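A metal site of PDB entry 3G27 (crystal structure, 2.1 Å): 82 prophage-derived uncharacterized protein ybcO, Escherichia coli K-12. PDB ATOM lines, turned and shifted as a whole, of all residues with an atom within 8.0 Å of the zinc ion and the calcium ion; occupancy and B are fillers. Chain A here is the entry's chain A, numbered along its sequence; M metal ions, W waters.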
ATOM      1  N   GLU A  12      22.641 -13.604  -2.407  1.00  0.00           N
ATOM      2  CA  GLU A  12      23.881 -14.142  -2.952  1.00  0.00           C
ATOM      3  C   GLU A  12      23.768 -14.625  -4.403  1.00  0.00           C
ATOM      4  O   GLU A  12      22.802 -15.296  -4.784  1.00  0.00           O
ATOM      5  CB  GLU A  12      24.321 -15.313  -2.071  1.00  0.00           C
ATOM      6  CG  GLU A  12      25.727 -15.801  -2.341  1.00  0.00           C
ATOM      7  CD  GLU A  12      26.519 -16.034  -1.051  1.00  0.00           C
ATOM      8  OE1 GLU A  12      26.345 -17.113  -0.404  1.00  0.00           O
ATOM      9  OE2 GLU A  12      27.308 -15.097  -0.725  1.00  0.00           O
ATOM     10  N   CYS A  13      24.800 -14.330  -5.194  1.00  0.00           N
ATOM     11  CA  CYS A  13      24.873 -14.787  -6.578  1.00  0.00           C
ATOM     12  C   CYS A  13      24.877 -16.301  -6.592  1.00  0.00           C
ATOM     13  O   CYS A  13      25.634 -16.923  -5.864  1.00  0.00           O
ATOM     14  CB  CYS A  13      26.152 -14.270  -7.244  1.00  0.00           C
ATOM     15  SG  CYS A  13      26.330 -14.644  -8.986  1.00  0.00           S
ATOM     16  N   GLN A  14      24.014 -16.884  -7.429  1.00  0.00           N
ATOM     17  CA  GLN A  14      23.972 -18.335  -7.609  1.00  0.00           C
ATOM     18  C   GLN A  14      24.706 -18.798  -8.858  1.00  0.00           C
ATOM     19  O   GLN A  14      24.816 -19.993  -9.080  1.00  0.00           O
ATOM     20  CB  GLN A  14      22.532 -18.812  -7.652  1.00  0.00           C
ATOM     21  CG  GLN A  14      21.756 -18.538  -6.392  1.00  0.00           C
ATOM     22  CD  GLN A  14      22.400 -19.213  -5.171  1.00  0.00           C
ATOM     23  OE1 GLN A  14      22.610 -20.427  -5.174  1.00  0.00           O
ATOM     24  NE2 GLN A  14      22.748 -18.427  -4.152  1.00  0.00           N
ATOM     25  N   VAL A  15      25.227 -17.869  -9.664  1.00  0.00           N
ATOM     26  CA  VAL A  15      25.924 -18.213 -10.930  1.00  0.00           C
ATOM     27  C   VAL A  15      27.387 -18.471 -10.613  1.00  0.00           C
ATOM     28  O   VAL A  15      27.946 -19.502 -10.968  1.00  0.00           O
ATOM     29  CB  VAL A  15      25.827 -17.085 -11.981  1.00  0.00           C
ATOM     30  CG1 VAL A  15      26.647 -17.432 -13.217  1.00  0.00           C
ATOM     31  CG2 VAL A  15      24.395 -16.793 -12.380  1.00  0.00           C
ATOM     32  N   ARG A  16      28.022 -17.502  -9.951  1.00  0.00           N
ATOM     33  CA  ARG A  16      29.376 -17.660  -9.419  1.00  0.00           C
ATOM     34  C   ARG A  16      30.425 -18.153 -10.428  1.00  0.00           C
ATOM     35  O   ARG A  16      31.145 -19.107 -10.141  1.00  0.00           O
ATOM     36  CB  ARG A  16      29.354 -18.588  -8.205  1.00  0.00           C
ATOM     37  CG  ARG A  16      28.087 -18.474  -7.355  1.00  0.00           C
ATOM     38  CD  ARG A  16      28.316 -18.975  -5.944  1.00  0.00           C
ATOM     39  NE  ARG A  16      27.093 -19.448  -5.293  1.00  0.00           N
ATOM     40  CZ  ARG A  16      26.768 -20.725  -5.179  1.00  0.00           C
ATOM     41  NH1 ARG A  16      25.640 -21.072  -4.563  1.00  0.00           N
ATOM     42  NH2 ARG A  16      27.570 -21.656  -5.681  1.00  0.00           N
ATOM     43  N   ILE A  17      30.518 -17.487 -11.582  1.00  0.00           N
ATOM     44  CA  ILE A  17      31.577 -17.802 -12.532  1.00  0.00           C
ATOM     45  C   ILE A  17      32.893 -17.378 -11.891  1.00  0.00           C
ATOM     46  O   ILE A  17      33.065 -16.204 -11.491  1.00  0.00           O
ATOM     47  CB  ILE A  17      31.397 -17.087 -13.892  1.00  0.00           C
ATOM     48  CG1 ILE A  17      30.098 -17.513 -14.551  1.00  0.00           C
ATOM     49  CG2 ILE A  17      32.592 -17.404 -14.783  1.00  0.00           C
ATOM     50  CD1 ILE A  17      29.666 -16.681 -15.729  1.00  0.00           C
ATOM     51  N   PRO A  18      33.842 -18.299 -11.767  1.00  0.00           N
ATOM     52  CA  PRO A  18      35.082 -17.900 -11.135  1.00  0.00           C
ATOM     53  C   PRO A  18      35.735 -16.696 -11.808  1.00  0.00           C
ATOM     54  O   PRO A  18      35.729 -16.596 -13.019  1.00  0.00           O
ATOM     55  CB  PRO A  18      35.964 -19.138 -11.273  1.00  0.00           C
ATOM     56  CG  PRO A  18      34.984 -20.276 -11.310  1.00  0.00           C
ATOM     57  CD  PRO A  18      33.826 -19.753 -12.070  1.00  0.00           C
ATOM     58  N   GLY A  19      36.286 -15.791 -11.006  1.00  0.00           N
ATOM     59  CA  GLY A  19      36.971 -14.622 -11.517  1.00  0.00           C
ATOM     60  C   GLY A  19      35.974 -13.540 -11.820  1.00  0.00           C
ATOM     61  O   GLY A  19      35.999 -12.450 -11.229  1.00  0.00           O
ATOM     62  N   VAL A  20      35.072 -13.869 -12.730  1.00  0.00           N
ATOM     63  CA  VAL A  20      34.012 -12.963 -13.156  1.00  0.00           C
ATOM     64  C   VAL A  20      33.098 -12.487 -12.000  1.00  0.00           C
ATOM     65  O   VAL A  20      32.786 -11.287 -11.872  1.00  0.00           O
ATOM     66  CB  VAL A  20      33.156 -13.622 -14.326  1.00  0.00           C
ATOM     67  CG1 VAL A  20      31.950 -12.777 -14.638  1.00  0.00           C
ATOM     68  CG2 VAL A  20      34.004 -13.872 -15.564  1.00  0.00           C
ATOM     69  N   CYS A  21      32.688 -13.414 -11.157  1.00  0.00           N
ATOM     70  CA  CYS A  21      31.824 -13.086 -10.034  1.00  0.00           C
ATOM     71  C   CYS A  21      32.441 -11.988  -9.211  1.00  0.00           C
ATOM     72  O   CYS A  21      33.654 -12.018  -8.935  1.00  0.00           O
ATOM     73  CB  CYS A  21      31.584 -14.314  -9.134  1.00  0.00           C
ATOM     74  SG  CYS A  21      30.041 -14.205  -8.067  1.00  0.00           S
ATOM     75  N   ASN A  22      31.627 -11.038  -8.792  1.00  0.00           N
ATOM     76  CA  ASN A  22      32.078 -10.068  -7.813  1.00  0.00           C
ATOM     77  C   ASN A  22      31.757 -10.487  -6.358  1.00  0.00           C
ATOM     78  O   ASN A  22      32.272  -9.914  -5.436  1.00  0.00           O
ATOM     79  CB  ASN A  22      31.601  -8.640  -8.152  1.00  0.00           C
ATOM     80  CG  ASN A  22      30.097  -8.447  -8.086  1.00  0.00           C
ATOM     81  OD1 ASN A  22      29.407  -9.002  -7.240  1.00  0.00           O
ATOM     82  ND2 ASN A  22      29.594  -7.631  -8.978  1.00  0.00           N
ATOM     83  N   GLY A  23      30.893 -11.466  -6.175  1.00  0.00           N
ATOM     84  CA  GLY A  23      30.538 -11.942  -4.846  1.00  0.00           C
ATOM     85  C   GLY A  23      29.817 -10.958  -3.942  1.00  0.00           C
ATOM     86  O   GLY A  23      29.780 -11.152  -2.709  1.00  0.00           O
ATOM     87  N   ASN A  24      29.258  -9.899  -4.524  1.00  0.00           N
ATOM     88  CA  ASN A  24      28.682  -8.819  -3.754  1.00  0.00           C
ATOM     89  C   ASN A  24      27.163  -8.856  -3.909  1.00  0.00           C
ATOM     90  O   ASN A  24      26.620  -8.402  -4.920  1.00  0.00           O
ATOM     91  CB  ASN A  24      29.282  -7.491  -4.172  1.00  0.00           C
ATOM     92  CG  ASN A  24      28.839  -6.358  -3.299  1.00  0.00           C
ATOM     93  OD1 ASN A  24      28.064  -6.521  -2.342  1.00  0.00           O
ATOM     94  ND2 ASN A  24      29.306  -5.178  -3.632  1.00  0.00           N
ATOM     95  N   THR A  27      24.738  -6.288  -5.433  1.00  0.00           N
ATOM     96  CA  THR A  27      24.603  -6.069  -6.884  1.00  0.00           C
ATOM     97  C   THR A  27      23.657  -7.090  -7.522  1.00  0.00           C
ATOM     98  O   THR A  27      23.446  -7.043  -8.737  1.00  0.00           O
ATOM     99  CB  THR A  27      25.967  -6.066  -7.571  1.00  0.00           C
ATOM    100  OG1 THR A  27      26.509  -7.385  -7.573  1.00  0.00           O
ATOM    101  CG2 THR A  27      26.923  -5.140  -6.848  1.00  0.00           C
ATOM    102  N   SER A  28      23.072  -7.997  -6.731  1.00  0.00           N
ATOM    103  CA  SER A  28      22.371  -9.145  -7.294  1.00  0.00           C
ATOM    104  C   SER A  28      21.073  -8.733  -7.877  1.00  0.00           C
ATOM    105  O   SER A  28      20.387  -7.901  -7.296  1.00  0.00           O
ATOM    106  CB  SER A  28      22.081 -10.200  -6.241  1.00  0.00           C
ATOM    107  OG  SER A  28      23.256 -10.967  -6.025  1.00  0.00           O
ATOM    108  N   ILE A  52      19.447 -15.666  -9.738  1.00  0.00           N
ATOM    109  CA  ILE A  52      20.032 -14.572  -8.966  1.00  0.00           C
ATOM    110  C   ILE A  52      21.456 -14.485  -9.496  1.00  0.00           C
ATOM    111  O   ILE A  52      22.160 -15.487  -9.565  1.00  0.00           O
ATOM    112  CB  ILE A  52      20.108 -14.881  -7.421  1.00  0.00           C
ATOM    113  CG1 ILE A  52      18.729 -15.305  -6.831  1.00  0.00           C
ATOM    114  CG2 ILE A  52      20.604 -13.709  -6.664  1.00  0.00           C
ATOM    115  CD1 ILE A  52      18.839 -16.024  -5.472  1.00  0.00           C
ATOM    116  N   ALA A  53      21.867 -13.285  -9.879  1.00  0.00           N
ATOM    117  CA  ALA A  53      23.188 -13.103 -10.439  1.00  0.00           C
ATOM    118  C   ALA A  53      23.666 -11.738  -9.996  1.00  0.00           C
ATOM    119  O   ALA A  53      22.892 -10.794 -10.003  1.00  0.00           O
ATOM    120  CB  ALA A  53      23.120 -13.189 -11.983  1.00  0.00           C
ATOM    121  N   CYS A  54      24.929 -11.662  -9.591  1.00  0.00           N
ATOM    122  CA  CYS A  54      25.618 -10.394  -9.344  1.00  0.00           C
ATOM    123  C   CYS A  54      25.818  -9.686 -10.659  1.00  0.00           C
ATOM    124  O   CYS A  54      25.684 -10.292 -11.713  1.00  0.00           O
ATOM    125  CB  CYS A  54      26.981 -10.607  -8.716  1.00  0.00           C
ATOM    126  SG  CYS A  54      28.258 -11.323  -9.828  1.00  0.00           S
ATOM    127  N   SER A  55      26.147  -8.392 -10.599  1.00  0.00           N
ATOM    128  CA  SER A  55      26.186  -7.558 -11.786  1.00  0.00           C
ATOM    129  C   SER A  55      27.130  -8.091 -12.855  1.00  0.00           C
ATOM    130  O   SER A  55      26.833  -8.045 -14.052  1.00  0.00           O
ATOM    131  CB  SER A  55      26.538  -6.111 -11.407  1.00  0.00           C
ATOM    132  OG  SER A  55      27.741  -6.018 -10.632  1.00  0.00           O
ATOM    133  N   ALA A  56      28.267  -8.627 -12.405  1.00  0.00           N
ATOM    134  CA  ALA A  56      29.306  -9.166 -13.276  1.00  0.00           C
ATOM    135  C   ALA A  56      28.878 -10.443 -13.963  1.00  0.00           C
ATOM    136  O   ALA A  56      29.039 -10.629 -15.160  1.00  0.00           O
ATOM    137  CB  ALA A  56      30.554  -9.420 -12.451  1.00  0.00           C
ATOM    138  N   CYS A  57      28.337 -11.354 -13.182  1.00  0.00           N
ATOM    139  CA  CYS A  57      27.869 -12.622 -13.741  1.00  0.00           C
ATOM    140  C   CYS A  57      26.700 -12.397 -14.679  1.00  0.00           C
ATOM    141  O   CYS A  57      26.589 -13.031 -15.710  1.00  0.00           O
ATOM    142  CB  CYS A  57      27.492 -13.591 -12.615  1.00  0.00           C
ATOM    143  SG  CYS A  57      28.901 -14.370 -11.835  1.00  0.00           S
ATOM    144  N   HIS A  58      25.828 -11.443 -14.354  1.00  0.00           N
ATOM    145  CA  HIS A  58      24.729 -11.108 -15.216  1.00  0.00           C
ATOM    146  C   HIS A  58      25.234 -10.658 -16.581  1.00  0.00           C
ATOM    147  O   HIS A  58      24.789 -11.146 -17.603  1.00  0.00           O
ATOM    148  CB  HIS A  58      23.933 -10.008 -14.543  1.00  0.00           C
ATOM    149  CG  HIS A  58      22.675  -9.640 -15.233  1.00  0.00           C
ATOM    150  ND1 HIS A  58      22.028  -8.451 -14.993  1.00  0.00           N
ATOM    151  CD2 HIS A  58      21.920 -10.315 -16.129  1.00  0.00           C
ATOM    152  CE1 HIS A  58      20.929  -8.415 -15.730  1.00  0.00           C
ATOM    153  NE2 HIS A  58      20.844  -9.533 -16.424  1.00  0.00           N
ATOM    154  N   ILE A  61      26.706 -13.806 -18.410  1.00  0.00           N
ATOM    155  CA  ILE A  61      25.764 -14.810 -18.874  1.00  0.00           C
ATOM    156  C   ILE A  61      24.938 -14.272 -20.053  1.00  0.00           C
ATOM    157  O   ILE A  61      24.528 -15.042 -20.910  1.00  0.00           O
ATOM    158  CB  ILE A  61      24.860 -15.426 -17.729  1.00  0.00           C
ATOM    159  CG1 ILE A  61      23.838 -14.423 -17.171  1.00  0.00           C
ATOM    160  CG2 ILE A  61      25.726 -16.062 -16.656  1.00  0.00           C
ATOM    161  CD1 ILE A  61      22.798 -15.035 -16.162  1.00  0.00           C
HETATM  162 ZN    ZN M   1      28.402 -13.649  -9.619  1.00  0.00          ZN
HETATM  163 CA    CA M   2      35.905 -11.079  -9.265  1.00  0.00          CA
HETATM  164  O   HOH W   1      35.477 -10.678  -6.967  1.00  0.00           O
HETATM  165  O   HOH W   2      35.978 -13.526  -8.305  1.00  0.00           O
HETATM  166  O   HOH W   3      34.259  -9.551 -10.507  1.00  0.00           O
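N of Gly 23 sits close to SG of Cys 21, at 3.4 Å.
The backbone NH of Asn 22 lies close to the side-chain sulfur of Cys 54 (3.5 Å).
The side-chain sulfur of Cys 54 lies close to the backbone NH of Ala 56 (3.7 Å).
The backbone NH of Arg 16 sits close to the side-chain sulfur of Cys 57, at 3.8 Å.
SG of Cys 57 sits close to N of Ile 17 (3.5 Å).
The backbone carbonyl oxygen (O) of Cys 13 is in hydrogen-bond range of the guanidinium group (NE) of Arg 16 (3.0 Å).
The backbone NH (N) of Val 15 sits close to the side-chain sulfur (SG) of Cys 13 (3.5 Å).
The side-chain amide oxygen (OE1) of Gln 14 sits at hydrogen-bond distance from the guanidinium group (NH1) of Arg 16.
Residues that only touch the zinc ion: Arg 16.
Within 4 Å of the zinc ion: Cys 13, Arg 16, Cys 21, Cys 54 and Cys 57.
The nearest printed residue that does not touch the zinc ion is Asn 22 (4.2 Å).
The zinc ion is bound by the side-chain sulfur (SG) of Cys 21, the side-chain sulfur (SG) of Cys 54, the side-chain sulfur (SG) of Cys 57 and the side-chain sulfur (SG) of Cys 13.
The calcium ion is bound by water W1, O of Gly 19, O of Cys 21, water W3 and water W2.
The calcium ion has five donor atoms within binding distance.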
